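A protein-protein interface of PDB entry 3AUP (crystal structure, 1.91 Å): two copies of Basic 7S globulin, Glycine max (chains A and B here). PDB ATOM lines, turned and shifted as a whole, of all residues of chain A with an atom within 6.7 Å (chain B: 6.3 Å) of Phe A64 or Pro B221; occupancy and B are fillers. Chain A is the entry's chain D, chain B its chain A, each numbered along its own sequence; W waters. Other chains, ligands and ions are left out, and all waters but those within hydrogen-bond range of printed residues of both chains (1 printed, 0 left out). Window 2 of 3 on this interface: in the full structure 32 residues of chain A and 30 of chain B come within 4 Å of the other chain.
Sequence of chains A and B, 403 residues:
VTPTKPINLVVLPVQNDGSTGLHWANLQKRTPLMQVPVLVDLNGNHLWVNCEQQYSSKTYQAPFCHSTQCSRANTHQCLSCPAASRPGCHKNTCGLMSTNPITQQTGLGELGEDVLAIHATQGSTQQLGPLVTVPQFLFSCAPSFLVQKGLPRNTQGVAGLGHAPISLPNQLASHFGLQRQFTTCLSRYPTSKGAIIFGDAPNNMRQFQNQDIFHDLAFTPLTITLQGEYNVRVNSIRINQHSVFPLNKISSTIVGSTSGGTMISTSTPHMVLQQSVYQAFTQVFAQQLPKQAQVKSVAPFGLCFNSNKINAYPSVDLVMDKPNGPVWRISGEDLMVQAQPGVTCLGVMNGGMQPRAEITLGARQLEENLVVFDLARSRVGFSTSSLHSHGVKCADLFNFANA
The side-chain hydroxyl of Ser B378 is in hydrogen-bond range of the backbone NH of Thr A68, 2.9 Å away.
Water W1 lies within hydrogen-bond range of the side-chain amide nitrogen (NE2) of Gln A69 and the backbone carbonyl oxygen (O) of Arg B377.
Along chain A the printed residues that touch a printed residue of chain B span positions 64 to 69. Hydrophobic or aromatic side chains of chain B within 4 Å of the printed part of chain A: Pro B221 and Leu B222. Among the printed residues, 11 pairs touch across the chains. Among the printed residues, no Asp or Glu carboxylate lies within 4 Å of a Lys or Arg side-chain nitrogen of the other chain.
No position is printed for both chains. Of the 11 pairs that touch across the chains among the printed residues, none has its exchanged pair printed and touching as well.
The side-chain sulfur of Cys A65 forms a disulfide with the side-chain sulfur of Cys A78, 2.0 Å away. The backbone NH of Cys A65 lies within hydrogen-bond range of the backbone carbonyl oxygen of Asn A92 (3.0 Å). The backbone NH (N) of Thr B223 is in hydrogen-bond range of the backbone carbonyl oxygen (O) of Asn B231. The side-chain sulfur (SG) of Cys A70 is in hydrogen-bond range of the side-chain hydroxyl (OG) of Ser A67, at 3.1 Å. O of Leu B222 sits at hydrogen-bond distance from OG of Ser B378, 2.7 Å away. The backbone carbonyl oxygen (O) of Phe A64 sits at hydrogen-bond distance from the side-chain hydroxyl (OG) of Ser A67, at 2.7 Å.
Among the printed residues, pairs that only touch across the chains: Phe A64 with Pro B221, Phe A64 with Leu B222, Phe A64 with Thr B223, Phe A64 with Ser B378, Cys A65 with Thr B223, His A66 with Thr B223, Ser A67 with Leu B222, Ser A67 with Ser B378, Thr A68 with Leu B222 and Gln A69 with Ser B378.
Phe A64 touches four residues of chain B. Of the printed residues of chain B, Cys A65 touches Thr B223 (3.98 Å). Printed residues of chain B within 4 Å of Gln A69: Ser B378 (3.3 Å). Of chain A, only Phe A64 (3.8 Å) comes within 4 Å of Pro B221. Of the printed residues of chain A, Ser B378 touches Phe A64 (3.6 Å), Ser A67 (3.3 Å), Thr A68 (2.9 Å) and Gln A69 (3.3 Å). The nearest printed residue of chain A that does not touch Pro B221 is Ser A67 (7.6 Å). The nearest printed residue of chain A that does not touch Thr B223 is Ser A67 (4.5 Å).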
ATOM      1  N   ALA A  62       7.207  -5.828  29.088  1.00  0.00           N
ATOM      2  CA  ALA A  62       7.228  -5.711  27.632  1.00  0.00           C
ATOM      3  C   ALA A  62       6.920  -7.102  27.074  1.00  0.00           C
ATOM      4  O   ALA A  62       7.684  -8.030  27.312  1.00  0.00           O
ATOM      5  CB  ALA A  62       8.555  -5.248  27.173  1.00  0.00           C
ATOM      6  N   PRO A  63       5.779  -7.263  26.366  1.00  0.00           N
ATOM      7  CA  PRO A  63       5.436  -8.581  25.851  1.00  0.00           C
ATOM      8  C   PRO A  63       6.501  -9.160  24.903  1.00  0.00           C
ATOM      9  O   PRO A  63       7.187  -8.413  24.212  1.00  0.00           O
ATOM     10  CB  PRO A  63       4.120  -8.323  25.129  1.00  0.00           C
ATOM     11  CG  PRO A  63       3.472  -7.220  25.936  1.00  0.00           C
ATOM     12  CD  PRO A  63       4.645  -6.321  26.254  1.00  0.00           C
ATOM     13  N   PHE A  64       6.642 -10.476  24.879  1.00  0.00           N
ATOM     14  CA  PHE A  64       7.648 -11.108  24.030  1.00  0.00           C
ATOM     15  C   PHE A  64       7.157 -11.239  22.586  1.00  0.00           C
ATOM     16  O   PHE A  64       5.942 -11.214  22.300  1.00  0.00           O
ATOM     17  CB  PHE A  64       8.135 -12.465  24.598  1.00  0.00           C
ATOM     18  CG  PHE A  64       7.033 -13.437  24.951  1.00  0.00           C
ATOM     19  CD1 PHE A  64       6.588 -13.573  26.281  1.00  0.00           C
ATOM     20  CD2 PHE A  64       6.456 -14.252  23.968  1.00  0.00           C
ATOM     21  CE1 PHE A  64       5.547 -14.478  26.603  1.00  0.00           C
ATOM     22  CE2 PHE A  64       5.435 -15.185  24.295  1.00  0.00           C
ATOM     23  CZ  PHE A  64       4.983 -15.286  25.600  1.00  0.00           C
ATOM     24  N   CYS A  65       8.095 -11.368  21.661  1.00  0.00           N
ATOM     25  CA  CYS A  65       7.705 -11.522  20.268  1.00  0.00           C
ATOM     26  C   CYS A  65       6.832 -12.751  20.036  1.00  0.00           C
ATOM     27  O   CYS A  65       7.040 -13.814  20.613  1.00  0.00           O
ATOM     28  CB  CYS A  65       8.901 -11.540  19.316  1.00  0.00           C
ATOM     29  SG  CYS A  65       8.463 -10.696  17.758  1.00  0.00           S
ATOM     30  N   HIS A  66       5.830 -12.557  19.186  1.00  0.00           N
ATOM     31  CA  HIS A  66       4.863 -13.587  18.790  1.00  0.00           C
ATOM     32  C   HIS A  66       3.853 -13.940  19.904  1.00  0.00           C
ATOM     33  O   HIS A  66       3.097 -14.908  19.778  1.00  0.00           O
ATOM     34  CB  HIS A  66       5.567 -14.845  18.285  1.00  0.00           C
ATOM     35  CG  HIS A  66       6.427 -14.639  17.069  1.00  0.00           C
ATOM     36  ND1 HIS A  66       6.064 -15.097  15.824  1.00  0.00           N
ATOM     37  CD2 HIS A  66       7.661 -14.102  16.923  1.00  0.00           C
ATOM     38  CE1 HIS A  66       7.024 -14.825  14.954  1.00  0.00           C
ATOM     39  NE2 HIS A  66       8.002 -14.215  15.596  1.00  0.00           N
ATOM     40  N   SER A  67       3.827 -13.138  20.973  1.00  0.00           N
ATOM     41  CA  SER A  67       2.906 -13.317  22.050  1.00  0.00           C
ATOM     42  C   SER A  67       1.500 -12.930  21.640  1.00  0.00           C
ATOM     43  O   SER A  67       1.244 -12.256  20.621  1.00  0.00           O
ATOM     44  CB  SER A  67       3.293 -12.442  23.258  1.00  0.00           C
ATOM     45  OG  SER A  67       3.315 -11.046  22.917  1.00  0.00           O
ATOM     46  N   THR A  68       0.585 -13.288  22.515  1.00  0.00           N
ATOM     47  CA  THR A  68      -0.801 -12.919  22.357  1.00  0.00           C
ATOM     48  C   THR A  68      -1.013 -11.428  22.363  1.00  0.00           C
ATOM     49  O   THR A  68      -1.798 -10.929  21.553  1.00  0.00           O
ATOM     50  CB  THR A  68      -1.701 -13.605  23.409  1.00  0.00           C
ATOM     51  OG1 THR A  68      -1.277 -13.236  24.714  1.00  0.00           O
ATOM     52  CG2 THR A  68      -1.629 -15.099  23.241  1.00  0.00           C
ATOM     53  N   GLN A  69      -0.300 -10.702  23.229  1.00  0.00           N
ATOM     54  CA  GLN A  69      -0.446  -9.255  23.271  1.00  0.00           C
ATOM     55  C   GLN A  69       0.035  -8.607  21.974  1.00  0.00           C
ATOM     56  O   GLN A  69      -0.611  -7.649  21.517  1.00  0.00           O
ATOM     57  CB  GLN A  69       0.278  -8.631  24.442  1.00  0.00           C
ATOM     58  CG  GLN A  69      -0.131  -9.207  25.785  1.00  0.00           C
ATOM     59  CD  GLN A  69       0.898 -10.143  26.361  1.00  0.00           C
ATOM     60  OE1 GLN A  69       1.448 -11.009  25.659  1.00  0.00           O
ATOM     61  NE2 GLN A  69       1.161  -9.990  27.655  1.00  0.00           N
ATOM     62  N   CYS A  70       1.144  -9.118  21.399  1.00  0.00           N
ATOM     63  CA  CYS A  70       1.678  -8.580  20.130  1.00  0.00           C
ATOM     64  C   CYS A  70       0.739  -8.875  18.965  1.00  0.00           C
ATOM     65  O   CYS A  70       0.571  -8.054  18.060  1.00  0.00           O
ATOM     66  CB  CYS A  70       3.081  -9.108  19.817  1.00  0.00           C
ATOM     67  SG  CYS A  70       4.141  -8.641  21.163  1.00  0.00           S
ATOM     68  N   CYS A  78       9.783  -8.331  15.490  1.00  0.00           N
ATOM     69  CA  CYS A  78      10.498  -8.554  16.751  1.00  0.00           C
ATOM     70  C   CYS A  78      11.592  -7.529  16.855  1.00  0.00           C
ATOM     71  O   CYS A  78      12.253  -7.250  15.866  1.00  0.00           O
ATOM     72  CB  CYS A  78      11.119  -9.943  16.817  1.00  0.00           C
ATOM     73  SG  CYS A  78       9.964 -11.265  16.608  1.00  0.00           S
ATOM     74  N   LYS A  91      15.322  -7.316  24.818  1.00  0.00           N
ATOM     75  CA  LYS A  91      15.563  -8.229  23.720  1.00  0.00           C
ATOM     76  C   LYS A  91      14.279  -9.003  23.490  1.00  0.00           C
ATOM     77  O   LYS A  91      13.486  -9.185  24.411  1.00  0.00           O
ATOM     78  CB  LYS A  91      16.746  -9.128  24.034  1.00  0.00           C
ATOM     79  CG  LYS A  91      18.053  -8.334  24.005  1.00  0.00           C
ATOM     80  CD  LYS A  91      19.131  -8.913  24.887  1.00  0.00           C
ATOM     81  CE  LYS A  91      20.374  -8.029  24.867  1.00  0.00           C
ATOM     82  NZ  LYS A  91      21.558  -8.806  25.293  1.00  0.00           N
ATOM     83  N   ASN A  92      14.044  -9.395  22.246  1.00  0.00           N
ATOM     84  CA  ASN A  92      12.877 -10.222  21.889  1.00  0.00           C
ATOM     85  C   ASN A  92      11.506  -9.633  22.262  1.00  0.00           C
ATOM     86  O   ASN A  92      10.656 -10.342  22.804  1.00  0.00           O
ATOM     87  CB  ASN A  92      13.048 -11.628  22.498  1.00  0.00           C
ATOM     88  CG  ASN A  92      12.141 -12.700  21.818  1.00  0.00           C
ATOM     89  OD1 ASN A  92      11.972 -12.717  20.585  1.00  0.00           O
ATOM     90  ND2 ASN A  92      11.581 -13.604  22.632  1.00  0.00           N
ATOM     91  N   THR A  93      11.275  -8.358  21.962  1.00  0.00           N
ATOM     92  CA  THR A  93       9.973  -7.761  22.197  1.00  0.00           C
ATOM     93  C   THR A  93       9.331  -7.406  20.822  1.00  0.00           C
ATOM     94  O   THR A  93       9.815  -7.886  19.803  1.00  0.00           O
ATOM     95  CB  THR A  93      10.095  -6.623  23.234  1.00  0.00           C
ATOM     96  OG1 THR A  93      11.133  -5.721  22.841  1.00  0.00           O
ATOM     97  CG2 THR A  93      10.417  -7.228  24.643  1.00  0.00           C
ATOM     98  N   CYS A  94       8.243  -6.638  20.796  1.00  0.00           N
ATOM     99  CA  CYS A  94       7.470  -6.407  19.585  1.00  0.00           C
ATOM    100  C   CYS A  94       7.533  -4.983  19.230  1.00  0.00           C
ATOM    101  O   CYS A  94       7.364  -4.133  20.081  1.00  0.00           O
ATOM    102  CB  CYS A  94       5.968  -6.778  19.813  1.00  0.00           C
ATOM    103  SG  CYS A  94       5.956  -8.365  20.451  1.00  0.00           S
ATOM    104  N   LEU A 111       6.173  -2.450  22.156  1.00  0.00           N
ATOM    105  CA  LEU A 111       4.917  -2.779  22.892  1.00  0.00           C
ATOM    106  C   LEU A 111       5.211  -2.938  24.412  1.00  0.00           C
ATOM    107  O   LEU A 111       6.129  -3.670  24.802  1.00  0.00           O
ATOM    108  CB  LEU A 111       4.253  -4.038  22.305  1.00  0.00           C
ATOM    109  CG  LEU A 111       2.779  -4.313  22.765  1.00  0.00           C
ATOM    110  CD1 LEU A 111       1.768  -3.271  22.239  1.00  0.00           C
ATOM    111  CD2 LEU A 111       2.341  -5.689  22.356  1.00  0.00           C
ATOM    112  N   PHE B 219       2.538 -23.396  33.931  1.00  0.00           N
ATOM    113  CA  PHE B 219       2.370 -22.496  32.808  1.00  0.00           C
ATOM    114  C   PHE B 219       3.547 -22.551  31.863  1.00  0.00           C
ATOM    115  O   PHE B 219       4.671 -22.762  32.298  1.00  0.00           O
ATOM    116  CB  PHE B 219       2.151 -21.082  33.326  1.00  0.00           C
ATOM    117  CG  PHE B 219       0.832 -20.913  34.026  1.00  0.00           C
ATOM    118  CD1 PHE B 219      -0.325 -20.753  33.300  1.00  0.00           C
ATOM    119  CD2 PHE B 219       0.749 -20.940  35.417  1.00  0.00           C
ATOM    120  CE1 PHE B 219      -1.568 -20.598  33.946  1.00  0.00           C
ATOM    121  CE2 PHE B 219      -0.494 -20.761  36.065  1.00  0.00           C
ATOM    122  CZ  PHE B 219      -1.639 -20.581  35.303  1.00  0.00           C
ATOM    123  N   THR B 220       3.275 -22.422  30.565  1.00  0.00           N
ATOM    124  CA  THR B 220       4.346 -22.320  29.552  1.00  0.00           C
ATOM    125  C   THR B 220       4.017 -21.192  28.554  1.00  0.00           C
ATOM    126  O   THR B 220       2.850 -20.901  28.291  1.00  0.00           O
ATOM    127  CB  THR B 220       4.633 -23.675  28.852  1.00  0.00           C
ATOM    128  OG1 THR B 220       5.918 -23.660  28.175  1.00  0.00           O
ATOM    129  CG2 THR B 220       3.567 -24.040  27.877  1.00  0.00           C
ATOM    130  N   PRO B 221       5.047 -20.506  28.024  1.00  0.00           N
ATOM    131  CA  PRO B 221       4.676 -19.395  27.150  1.00  0.00           C
ATOM    132  C   PRO B 221       3.903 -19.805  25.895  1.00  0.00           C
ATOM    133  O   PRO B 221       4.105 -20.913  25.341  1.00  0.00           O
ATOM    134  CB  PRO B 221       6.022 -18.760  26.789  1.00  0.00           C
ATOM    135  CG  PRO B 221       6.931 -19.144  27.885  1.00  0.00           C
ATOM    136  CD  PRO B 221       6.440 -20.419  28.476  1.00  0.00           C
ATOM    137  N   LEU B 222       2.994 -18.919  25.500  1.00  0.00           N
ATOM    138  CA  LEU B 222       2.137 -19.100  24.356  1.00  0.00           C
ATOM    139  C   LEU B 222       2.500 -18.094  23.265  1.00  0.00           C
ATOM    140  O   LEU B 222       2.663 -16.906  23.536  1.00  0.00           O
ATOM    141  CB  LEU B 222       0.673 -18.880  24.789  1.00  0.00           C
ATOM    142  CG  LEU B 222      -0.467 -19.006  23.782  1.00  0.00           C
ATOM    143  CD1 LEU B 222      -0.532 -20.373  23.050  1.00  0.00           C
ATOM    144  CD2 LEU B 222      -1.862 -18.710  24.483  1.00  0.00           C
ATOM    145  N   THR B 223       2.650 -18.592  22.042  1.00  0.00           N
ATOM    146  CA  THR B 223       2.807 -17.755  20.851  1.00  0.00           C
ATOM    147  C   THR B 223       1.652 -18.022  19.895  1.00  0.00           C
ATOM    148  O   THR B 223       0.897 -18.979  20.071  1.00  0.00           O
ATOM    149  CB  THR B 223       4.171 -17.957  20.196  1.00  0.00           C
ATOM    150  OG1 THR B 223       4.413 -19.353  20.023  1.00  0.00           O
ATOM    151  CG2 THR B 223       5.313 -17.370  21.086  1.00  0.00           C
ATOM    152  N   ASN B 231       0.659 -21.847  19.598  1.00  0.00           N
ATOM    153  CA  ASN B 231       1.884 -22.601  19.678  1.00  0.00           C
ATOM    154  C   ASN B 231       2.481 -22.516  21.093  1.00  0.00           C
ATOM    155  O   ASN B 231       2.351 -21.476  21.793  1.00  0.00           O
ATOM    156  CB  ASN B 231       2.881 -22.021  18.698  1.00  0.00           C
ATOM    157  CG  ASN B 231       2.896 -22.710  17.361  1.00  0.00           C
ATOM    158  OD1 ASN B 231       3.937 -22.693  16.701  1.00  0.00           O
ATOM    159  ND2 ASN B 231       1.779 -23.326  16.940  1.00  0.00           N
ATOM    160  N   VAL B 232       3.097 -23.629  21.518  1.00  0.00           N
ATOM    161  CA  VAL B 232       3.914 -23.685  22.728  1.00  0.00           C
ATOM    162  C   VAL B 232       5.253 -24.241  22.275  1.00  0.00           C
ATOM    163  O   VAL B 232       5.430 -24.545  21.102  1.00  0.00           O
ATOM    164  CB  VAL B 232       3.323 -24.594  23.846  1.00  0.00           C
ATOM    165  CG1 VAL B 232       2.009 -23.984  24.383  1.00  0.00           C
ATOM    166  CG2 VAL B 232       3.155 -25.986  23.333  1.00  0.00           C
ATOM    167  N   ARG B 233       6.212 -24.341  23.175  1.00  0.00           N
ATOM    168  CA  ARG B 233       7.526 -24.849  22.771  1.00  0.00           C
ATOM    169  C   ARG B 233       7.894 -26.019  23.625  1.00  0.00           C
ATOM    170  O   ARG B 233       7.927 -25.891  24.847  1.00  0.00           O
ATOM    171  CB  ARG B 233       8.608 -23.791  22.899  1.00  0.00           C
ATOM    172  CG  ARG B 233       9.915 -24.192  22.137  1.00  0.00           C
ATOM    173  CD  ARG B 233      11.226 -23.453  22.514  1.00  0.00           C
ATOM    174  NE  ARG B 233      11.029 -22.342  23.432  1.00  0.00           N
ATOM    175  CZ  ARG B 233      12.004 -21.666  24.027  1.00  0.00           C
ATOM    176  NH1 ARG B 233      11.704 -20.668  24.854  1.00  0.00           N
ATOM    177  NH2 ARG B 233      13.278 -21.964  23.801  1.00  0.00           N
ATOM    178  N   ASP B 321       9.000 -25.327  27.285  1.00  0.00           N
ATOM    179  CA  ASP B 321       9.719 -24.053  27.286  1.00  0.00           C
ATOM    180  C   ASP B 321      11.230 -24.268  27.262  1.00  0.00           C
ATOM    181  O   ASP B 321      11.901 -23.837  26.328  1.00  0.00           O
ATOM    182  CB  ASP B 321       9.277 -23.181  28.478  1.00  0.00           C
ATOM    183  CG  ASP B 321       9.958 -21.822  28.511  1.00  0.00           C
ATOM    184  OD1 ASP B 321      10.189 -21.238  27.423  1.00  0.00           O
ATOM    185  OD2 ASP B 321      10.228 -21.326  29.641  1.00  0.00           O
ATOM    186  N   ARG B 377      -2.076 -12.843  29.433  1.00  0.00           N
ATOM    187  CA  ARG B 377      -0.694 -13.038  29.884  1.00  0.00           C
ATOM    188  C   ARG B 377       0.181 -13.904  28.942  1.00  0.00           C
ATOM    189  O   ARG B 377       1.365 -14.145  29.221  1.00  0.00           O
ATOM    190  CB  ARG B 377      -0.711 -13.632  31.293  1.00  0.00           C
ATOM    191  CG  ARG B 377      -0.902 -12.565  32.385  1.00  0.00           C
ATOM    192  CD  ARG B 377      -0.839 -13.173  33.793  1.00  0.00           C
ATOM    193  N   SER B 378      -0.403 -14.344  27.836  1.00  0.00           N
ATOM    194  CA  SER B 378       0.287 -15.132  26.828  1.00  0.00           C
ATOM    195  C   SER B 378       0.919 -16.406  27.347  1.00  0.00           C
ATOM    196  O   SER B 378       2.128 -16.615  27.248  1.00  0.00           O
ATOM    197  CB  SER B 378       1.383 -14.291  26.145  1.00  0.00           C
ATOM    198  OG  SER B 378       1.564 -14.758  24.801  1.00  0.00           O
ATOM    199  N   ARG B 379       0.117 -17.259  27.930  1.00  0.00           N
ATOM    200  CA  ARG B 379       0.624 -18.518  28.443  1.00  0.00           C
ATOM    201  C   ARG B 379      -0.498 -19.530  28.384  1.00  0.00           C
ATOM    202  O   ARG B 379      -1.679 -19.157  28.381  1.00  0.00           O
ATOM    203  CB  ARG B 379       1.130 -18.352  29.881  1.00  0.00           C
ATOM    204  CG  ARG B 379       0.071 -17.911  30.866  1.00  0.00           C
ATOM    205  CD  ARG B 379       0.680 -17.581  32.220  1.00  0.00           C
ATOM    206  NE  ARG B 379      -0.352 -17.343  33.231  1.00  0.00           N
ATOM    207  CZ  ARG B 379      -0.103 -17.209  34.532  1.00  0.00           C
ATOM    208  NH1 ARG B 379       1.137 -17.276  35.003  1.00  0.00           N
ATOM    209  NH2 ARG B 379      -1.097 -16.996  35.371  1.00  0.00           N
ATOM    210  N   VAL B 380      -0.107 -20.794  28.295  1.00  0.00           N
ATOM    211  CA  VAL B 380      -1.017 -21.910  28.354  1.00  0.00           C
ATOM    212  C   VAL B 380      -0.770 -22.520  29.703  1.00  0.00           C
ATOM    213  O   VAL B 380       0.401 -22.744  30.085  1.00  0.00           O
ATOM    214  CB  VAL B 380      -0.666 -22.945  27.266  1.00  0.00           C
ATOM    215  CG1 VAL B 380      -1.500 -24.223  27.417  1.00  0.00           C
ATOM    216  CG2 VAL B 380      -0.886 -22.359  25.899  1.00  0.00           C
HETATM  217  O   HOH W   1       2.181 -11.231  30.086  1.00  0.00           O
